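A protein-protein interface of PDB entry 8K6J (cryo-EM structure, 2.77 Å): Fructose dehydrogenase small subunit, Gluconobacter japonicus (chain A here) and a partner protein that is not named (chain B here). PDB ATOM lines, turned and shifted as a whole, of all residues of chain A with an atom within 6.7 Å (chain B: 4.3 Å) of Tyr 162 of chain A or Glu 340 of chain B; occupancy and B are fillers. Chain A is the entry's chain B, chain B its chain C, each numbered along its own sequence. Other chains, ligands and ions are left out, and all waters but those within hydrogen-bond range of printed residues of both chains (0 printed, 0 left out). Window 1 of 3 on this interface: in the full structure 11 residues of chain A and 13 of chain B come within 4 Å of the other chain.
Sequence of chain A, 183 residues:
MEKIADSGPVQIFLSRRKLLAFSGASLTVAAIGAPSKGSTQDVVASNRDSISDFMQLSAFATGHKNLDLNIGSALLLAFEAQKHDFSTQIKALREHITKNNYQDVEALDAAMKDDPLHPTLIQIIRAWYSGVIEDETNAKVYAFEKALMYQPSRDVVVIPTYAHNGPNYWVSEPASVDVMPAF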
ATOM      1  N   PHE A 144      -8.845 -28.080  33.408  1.00  0.00           N
ATOM      2  CA  PHE A 144      -8.091 -26.908  32.988  1.00  0.00           C
ATOM      3  C   PHE A 144      -8.321 -26.700  31.501  1.00  0.00           C
ATOM      4  O   PHE A 144      -8.443 -27.670  30.746  1.00  0.00           O
ATOM      5  CB  PHE A 144      -6.597 -27.054  33.272  1.00  0.00           C
ATOM      6  CG  PHE A 144      -5.791 -25.850  32.884  1.00  0.00           C
ATOM      7  CD1 PHE A 144      -6.104 -24.601  33.387  1.00  0.00           C
ATOM      8  CD2 PHE A 144      -4.724 -25.965  32.015  1.00  0.00           C
ATOM      9  CE1 PHE A 144      -5.365 -23.493  33.031  1.00  0.00           C
ATOM     10  CE2 PHE A 144      -3.984 -24.859  31.657  1.00  0.00           C
ATOM     11  CZ  PHE A 144      -4.305 -23.622  32.167  1.00  0.00           C
ATOM     12  N   GLU A 145      -8.415 -25.433  31.096  1.00  0.00           N
ATOM     13  CA  GLU A 145      -8.692 -25.028  29.719  1.00  0.00           C
ATOM     14  C   GLU A 145     -10.126 -25.391  29.345  1.00  0.00           C
ATOM     15  O   GLU A 145     -10.605 -25.042  28.262  1.00  0.00           O
ATOM     16  CB  GLU A 145      -7.682 -25.654  28.750  1.00  0.00           C
ATOM     17  CG  GLU A 145      -7.703 -25.082  27.341  1.00  0.00           C
ATOM     18  CD  GLU A 145      -8.088 -26.107  26.297  1.00  0.00           C
ATOM     19  OE1 GLU A 145      -8.488 -25.702  25.186  1.00  0.00           O
ATOM     20  OE2 GLU A 145      -7.989 -27.317  26.585  1.00  0.00           O
ATOM     21  N   ARG A 154     -12.132 -16.212  27.402  1.00  0.00           N
ATOM     22  CA  ARG A 154     -11.451 -17.070  26.440  1.00  0.00           C
ATOM     23  C   ARG A 154     -11.222 -16.361  25.114  1.00  0.00           C
ATOM     24  O   ARG A 154     -10.238 -16.643  24.422  1.00  0.00           O
ATOM     25  CB  ARG A 154     -12.257 -18.348  26.220  1.00  0.00           C
ATOM     26  CG  ARG A 154     -11.421 -19.582  25.961  1.00  0.00           C
ATOM     27  CD  ARG A 154     -12.252 -20.646  25.262  1.00  0.00           C
ATOM     28  NE  ARG A 154     -11.953 -22.004  25.704  1.00  0.00           N
ATOM     29  CZ  ARG A 154     -10.768 -22.594  25.617  1.00  0.00           C
ATOM     30  NH1 ARG A 154      -9.730 -21.990  25.062  1.00  0.00           N
ATOM     31  NH2 ARG A 154     -10.626 -23.831  26.080  1.00  0.00           N
ATOM     32  N   VAL A 158      -5.619 -15.203  27.050  1.00  0.00           N
ATOM     33  CA  VAL A 158      -5.147 -16.535  26.696  1.00  0.00           C
ATOM     34  C   VAL A 158      -5.155 -17.418  27.934  1.00  0.00           C
ATOM     35  O   VAL A 158      -4.611 -17.048  28.980  1.00  0.00           O
ATOM     36  CB  VAL A 158      -3.742 -16.464  26.083  1.00  0.00           C
ATOM     37  CG1 VAL A 158      -2.911 -15.427  26.806  1.00  0.00           C
ATOM     38  CG2 VAL A 158      -3.063 -17.817  26.153  1.00  0.00           C
ATOM     39  N   ILE A 159      -5.782 -18.585  27.825  1.00  0.00           N
ATOM     40  CA  ILE A 159      -5.611 -19.631  28.827  1.00  0.00           C
ATOM     41  C   ILE A 159      -4.139 -20.013  28.770  1.00  0.00           C
ATOM     42  O   ILE A 159      -3.706 -20.624  27.785  1.00  0.00           O
ATOM     43  CB  ILE A 159      -6.526 -20.831  28.556  1.00  0.00           C
ATOM     44  CG1 ILE A 159      -7.988 -20.399  28.629  1.00  0.00           C
ATOM     45  CG2 ILE A 159      -6.246 -21.936  29.551  1.00  0.00           C
ATOM     46  CD1 ILE A 159      -8.948 -21.539  28.760  1.00  0.00           C
ATOM     47  N   PRO A 160      -3.352 -19.699  29.803  1.00  0.00           N
ATOM     48  CA  PRO A 160      -1.901 -19.536  29.629  1.00  0.00           C
ATOM     49  C   PRO A 160      -1.185 -20.593  28.800  1.00  0.00           C
ATOM     50  O   PRO A 160      -0.649 -20.272  27.738  1.00  0.00           O
ATOM     51  CB  PRO A 160      -1.394 -19.542  31.072  1.00  0.00           C
ATOM     52  CG  PRO A 160      -2.504 -18.921  31.836  1.00  0.00           C
ATOM     53  CD  PRO A 160      -3.778 -19.380  31.175  1.00  0.00           C
ATOM     54  N   THR A 161      -1.198 -21.854  29.218  1.00  0.00           N
ATOM     55  CA  THR A 161      -0.365 -22.832  28.531  1.00  0.00           C
ATOM     56  C   THR A 161      -0.813 -23.040  27.086  1.00  0.00           C
ATOM     57  O   THR A 161       0.021 -23.185  26.187  1.00  0.00           O
ATOM     58  CB  THR A 161      -0.361 -24.148  29.298  1.00  0.00           C
ATOM     59  OG1 THR A 161       0.358 -23.975  30.524  1.00  0.00           O
ATOM     60  CG2 THR A 161       0.319 -25.214  28.492  1.00  0.00           C
ATOM     61  N   TYR A 162      -2.119 -23.028  26.840  1.00  0.00           N
ATOM     62  CA  TYR A 162      -2.640 -23.261  25.499  1.00  0.00           C
ATOM     63  C   TYR A 162      -2.635 -21.971  24.692  1.00  0.00           C
ATOM     64  O   TYR A 162      -3.080 -20.925  25.170  1.00  0.00           O
ATOM     65  CB  TYR A 162      -4.047 -23.841  25.578  1.00  0.00           C
ATOM     66  CG  TYR A 162      -4.079 -25.194  26.238  1.00  0.00           C
ATOM     67  CD1 TYR A 162      -4.145 -25.312  27.616  1.00  0.00           C
ATOM     68  CD2 TYR A 162      -4.020 -26.353  25.484  1.00  0.00           C
ATOM     69  CE1 TYR A 162      -4.165 -26.544  28.222  1.00  0.00           C
ATOM     70  CE2 TYR A 162      -4.040 -27.590  26.081  1.00  0.00           C
ATOM     71  CZ  TYR A 162      -4.112 -27.680  27.451  1.00  0.00           C
ATOM     72  OH  TYR A 162      -4.133 -28.916  28.051  1.00  0.00           O
ATOM     73  N   ALA A 163      -2.143 -22.053  23.461  1.00  0.00           N
ATOM     74  CA  ALA A 163      -1.915 -20.862  22.659  1.00  0.00           C
ATOM     75  C   ALA A 163      -3.211 -20.314  22.077  1.00  0.00           C
ATOM     76  O   ALA A 163      -4.153 -21.054  21.782  1.00  0.00           O
ATOM     77  CB  ALA A 163      -0.940 -21.166  21.527  1.00  0.00           C
ATOM     78  N   HIS A 164      -3.246 -18.997  21.910  1.00  0.00           N
ATOM     79  CA  HIS A 164      -4.275 -18.337  21.120  1.00  0.00           C
ATOM     80  C   HIS A 164      -3.892 -18.448  19.643  1.00  0.00           C
ATOM     81  O   HIS A 164      -2.947 -19.149  19.276  1.00  0.00           O
ATOM     82  CB  HIS A 164      -4.442 -16.892  21.574  1.00  0.00           C
ATOM     83  CG  HIS A 164      -5.846 -16.523  21.935  1.00  0.00           C
ATOM     84  ND1 HIS A 164      -6.483 -15.420  21.410  1.00  0.00           N
ATOM     85  CD2 HIS A 164      -6.733 -17.105  22.775  1.00  0.00           C
ATOM     86  CE1 HIS A 164      -7.704 -15.341  21.906  1.00  0.00           C
ATOM     87  NE2 HIS A 164      -7.880 -16.351  22.738  1.00  0.00           N
ATOM     88  N   TYR B 315      -8.086 -36.334  26.043  1.00  0.00           N
ATOM     89  CA  TYR B 315      -7.527 -36.943  27.236  1.00  0.00           C
ATOM     90  C   TYR B 315      -8.353 -36.554  28.460  1.00  0.00           C
ATOM     91  O   TYR B 315      -9.325 -35.800  28.373  1.00  0.00           O
ATOM     92  CB  TYR B 315      -6.057 -36.544  27.389  1.00  0.00           C
ATOM     93  CG  TYR B 315      -5.782 -35.321  28.237  1.00  0.00           C
ATOM     94  CD1 TYR B 315      -6.378 -34.100  27.959  1.00  0.00           C
ATOM     95  CD2 TYR B 315      -4.887 -35.385  29.296  1.00  0.00           C
ATOM     96  CE1 TYR B 315      -6.119 -32.988  28.734  1.00  0.00           C
ATOM     97  CE2 TYR B 315      -4.615 -34.278  30.070  1.00  0.00           C
ATOM     98  CZ  TYR B 315      -5.231 -33.083  29.785  1.00  0.00           C
ATOM     99  OH  TYR B 315      -4.961 -31.978  30.557  1.00  0.00           O
ATOM    100  N   ALA B 336      -2.800 -40.065  24.644  1.00  0.00           N
ATOM    101  CA  ALA B 336      -3.517 -38.800  24.747  1.00  0.00           C
ATOM    102  C   ALA B 336      -2.806 -37.839  25.691  1.00  0.00           C
ATOM    103  O   ALA B 336      -2.684 -36.645  25.396  1.00  0.00           O
ATOM    104  CB  ALA B 336      -4.948 -39.051  25.212  1.00  0.00           C
ATOM    105  N   ALA B 337      -2.330 -38.342  26.830  1.00  0.00           N
ATOM    106  CA  ALA B 337      -1.606 -37.493  27.768  1.00  0.00           C
ATOM    107  C   ALA B 337      -0.311 -36.978  27.158  1.00  0.00           C
ATOM    108  O   ALA B 337       0.052 -35.813  27.348  1.00  0.00           O
ATOM    109  CB  ALA B 337      -1.324 -38.258  29.059  1.00  0.00           C
ATOM    110  N   LEU B 338       0.404 -37.836  26.427  1.00  0.00           N
ATOM    111  CA  LEU B 338       1.632 -37.402  25.771  1.00  0.00           C
ATOM    112  C   LEU B 338       1.350 -36.319  24.739  1.00  0.00           C
ATOM    113  O   LEU B 338       2.070 -35.316  24.669  1.00  0.00           O
ATOM    114  CB  LEU B 338       2.325 -38.592  25.114  1.00  0.00           C
ATOM    115  CG  LEU B 338       3.328 -39.360  25.971  1.00  0.00           C
ATOM    116  CD1 LEU B 338       3.702 -40.663  25.297  1.00  0.00           C
ATOM    117  CD2 LEU B 338       4.559 -38.518  26.228  1.00  0.00           C
ATOM    118  N   TYR B 339       0.301 -36.500  23.933  1.00  0.00           N
ATOM    119  CA  TYR B 339      -0.047 -35.482  22.950  1.00  0.00           C
ATOM    120  C   TYR B 339      -0.414 -34.172  23.626  1.00  0.00           C
ATOM    121  O   TYR B 339      -0.016 -33.095  23.168  1.00  0.00           O
ATOM    122  CB  TYR B 339      -1.198 -35.964  22.070  1.00  0.00           C
ATOM    123  CG  TYR B 339      -1.786 -34.874  21.204  1.00  0.00           C
ATOM    124  CD1 TYR B 339      -1.196 -34.529  19.999  1.00  0.00           C
ATOM    125  CD2 TYR B 339      -2.927 -34.188  21.592  1.00  0.00           C
ATOM    126  CE1 TYR B 339      -1.725 -33.536  19.208  1.00  0.00           C
ATOM    127  CE2 TYR B 339      -3.460 -33.193  20.806  1.00  0.00           C
ATOM    128  CZ  TYR B 339      -2.856 -32.871  19.616  1.00  0.00           C
ATOM    129  OH  TYR B 339      -3.386 -31.880  18.829  1.00  0.00           O
ATOM    130  N   GLU B 340      -1.179 -34.239  24.716  1.00  0.00           N
ATOM    131  CA  GLU B 340      -1.566 -33.018  25.408  1.00  0.00           C
ATOM    132  C   GLU B 340      -0.356 -32.308  25.999  1.00  0.00           C
ATOM    133  O   GLU B 340      -0.262 -31.077  25.947  1.00  0.00           O
ATOM    134  CB  GLU B 340      -2.587 -33.324  26.497  1.00  0.00           C
ATOM    135  CG  GLU B 340      -3.200 -32.083  27.104  1.00  0.00           C
ATOM    136  CD  GLU B 340      -4.353 -31.550  26.285  1.00  0.00           C
ATOM    137  OE1 GLU B 340      -4.677 -32.157  25.243  1.00  0.00           O
ATOM    138  OE2 GLU B 340      -4.944 -30.526  26.685  1.00  0.00           O
ATOM    139  N   ALA B 341       0.579 -33.068  26.568  1.00  0.00           N
ATOM    140  CA  ALA B 341       1.742 -32.449  27.189  1.00  0.00           C
ATOM    141  C   ALA B 341       2.672 -31.841  26.149  1.00  0.00           C
ATOM    142  O   ALA B 341       3.202 -30.742  26.351  1.00  0.00           O
ATOM    143  CB  ALA B 341       2.487 -33.472  28.042  1.00  0.00           C
ATOM    144  N   VAL B 342       2.880 -32.526  25.031  1.00  0.00           N
ATOM    145  CA  VAL B 342       3.899 -32.139  24.063  1.00  0.00           C
ATOM    146  C   VAL B 342       3.329 -31.272  22.949  1.00  0.00           C
ATOM    147  O   VAL B 342       3.892 -30.230  22.616  1.00  0.00           O
ATOM    148  CB  VAL B 342       4.597 -33.391  23.491  1.00  0.00           C
ATOM    149  CG1 VAL B 342       5.726 -32.986  22.572  1.00  0.00           C
ATOM    150  CG2 VAL B 342       5.113 -34.265  24.613  1.00  0.00           C
ATOM    151  N   ALA B 344      -0.277 -30.358  22.346  1.00  0.00           N
ATOM    152  CA  ALA B 344      -1.555 -29.663  22.428  1.00  0.00           C
ATOM    153  C   ALA B 344      -1.417 -28.163  22.629  1.00  0.00           C
ATOM    154  O   ALA B 344      -2.420 -27.451  22.513  1.00  0.00           O
ATOM    155  CB  ALA B 344      -2.411 -30.237  23.551  1.00  0.00           C
ATOM    156  N   SER B 345      -0.220 -27.665  22.937  1.00  0.00           N
ATOM    157  CA  SER B 345      -0.057 -26.231  23.141  1.00  0.00           C
ATOM    158  C   SER B 345      -0.353 -25.452  21.866  1.00  0.00           C
ATOM    159  O   SER B 345      -1.007 -24.405  21.908  1.00  0.00           O
ATOM    160  CB  SER B 345       1.354 -25.929  23.634  1.00  0.00           C
ATOM    161  OG  SER B 345       1.516 -24.544  23.873  1.00  0.00           O
ATOM    162  N   GLN B 348      -4.583 -27.336  19.027  1.00  0.00           N
ATOM    163  CA  GLN B 348      -5.433 -27.374  20.206  1.00  0.00           C
ATOM    164  C   GLN B 348      -5.758 -28.815  20.599  1.00  0.00           C
ATOM    165  O   GLN B 348      -5.507 -29.769  19.859  1.00  0.00           O
ATOM    166  CB  GLN B 348      -6.713 -26.581  19.960  1.00  0.00           C
ATOM    167  CG  GLN B 348      -6.478 -25.112  19.676  1.00  0.00           C
ATOM    168  CD  GLN B 348      -5.377 -24.527  20.533  1.00  0.00           C
ATOM    169  OE1 GLN B 348      -4.331 -24.124  20.031  1.00  0.00           O
ATOM    170  NE2 GLN B 348      -5.611 -24.474  21.836  1.00  0.00           N
ATOM    171  N   SER B 349      -6.328 -28.961  21.799  1.00  0.00           N
ATOM    172  CA  SER B 349      -6.586 -30.289  22.346  1.00  0.00           C
ATOM    173  C   SER B 349      -7.470 -31.122  21.429  1.00  0.00           C
ATOM    174  O   SER B 349      -7.330 -32.349  21.383  1.00  0.00           O
ATOM    175  CB  SER B 349      -7.225 -30.170  23.728  1.00  0.00           C
ATOM    176  OG  SER B 349      -6.918 -31.299  24.525  1.00  0.00           O
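Of the 10 printed residues of chain A, 3 touch a printed residue of chain B.
Printed residues of chain B that touch a printed residue of chain A: Glu 340, Ala 344, Ser 345 and Gln 348.
Along chain B the printed residues that touch a printed residue of chain A span positions 340 to 348.
Among the printed residues, no Asp or Glu carboxylate lies within 4 Å of a Lys or Arg side-chain nitrogen of the other chain.
Tyr 162 of chain A touches Ala 344 of chain B (CD2 to O, 3.5 Å).
Ala 163 of chain A touches Gln 348 of chain B (O to OE1, 3.5 Å).
Ile 159 of chain A touches none of the printed residues of chain B.
Of chain B, only Glu 340 and Ala 344 come within 4 Å of Tyr 162 of chain A.
Of the printed residues of chain B, Ala 163 of chain A touches Ser 345 (3.0 Å) and Gln 348 (3.5 Å).
Glu 340 of chain B touches one residue of chain A.
Val 342 of chain B touches none of the printed residues of chain A.
Printed residues of chain A within 4 Å of Ser 345 of chain B: Thr 161 and Ala 163.
Printed residues of chain A within 4 Å of Gln 348 of chain B: Ala 163.
The nearest printed residue of chain B that does not touch Tyr 162 of chain A is Ser 345 of chain B (4.04 Å).
The nearest residue of chain A that does not touch Glu 340 of chain B is Glu 145 of chain A (4.4 Å).
The backbone carbonyl oxygen (O) of Tyr 339 of chain B lies within hydrogen-bond range of the backbone NH (N) of Ala 344 of chain B (2.9 Å).
OH of Tyr 339 of chain B sits at hydrogen-bond distance from O of Gln 348 of chain B, at 3.2 Å.
The side-chain carboxylate of Glu 340 of chain B sits at hydrogen-bond distance from the side-chain hydroxyl of Ser 349 of chain B (2.5 Å).
OG of Ser 345 of chain B lies within hydrogen-bond range of O of Thr 161 of chain A, at 3.1 Å.
O of Ser 345 of chain B sits at hydrogen-bond distance from N of Ala 163 of chain A, 3.0 Å away.
The side-chain hydroxyl (OH) of Tyr 162 of chain A sits close to the side-chain carboxylate (OE2) of Glu 340 of chain B, 2.3 Å away.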
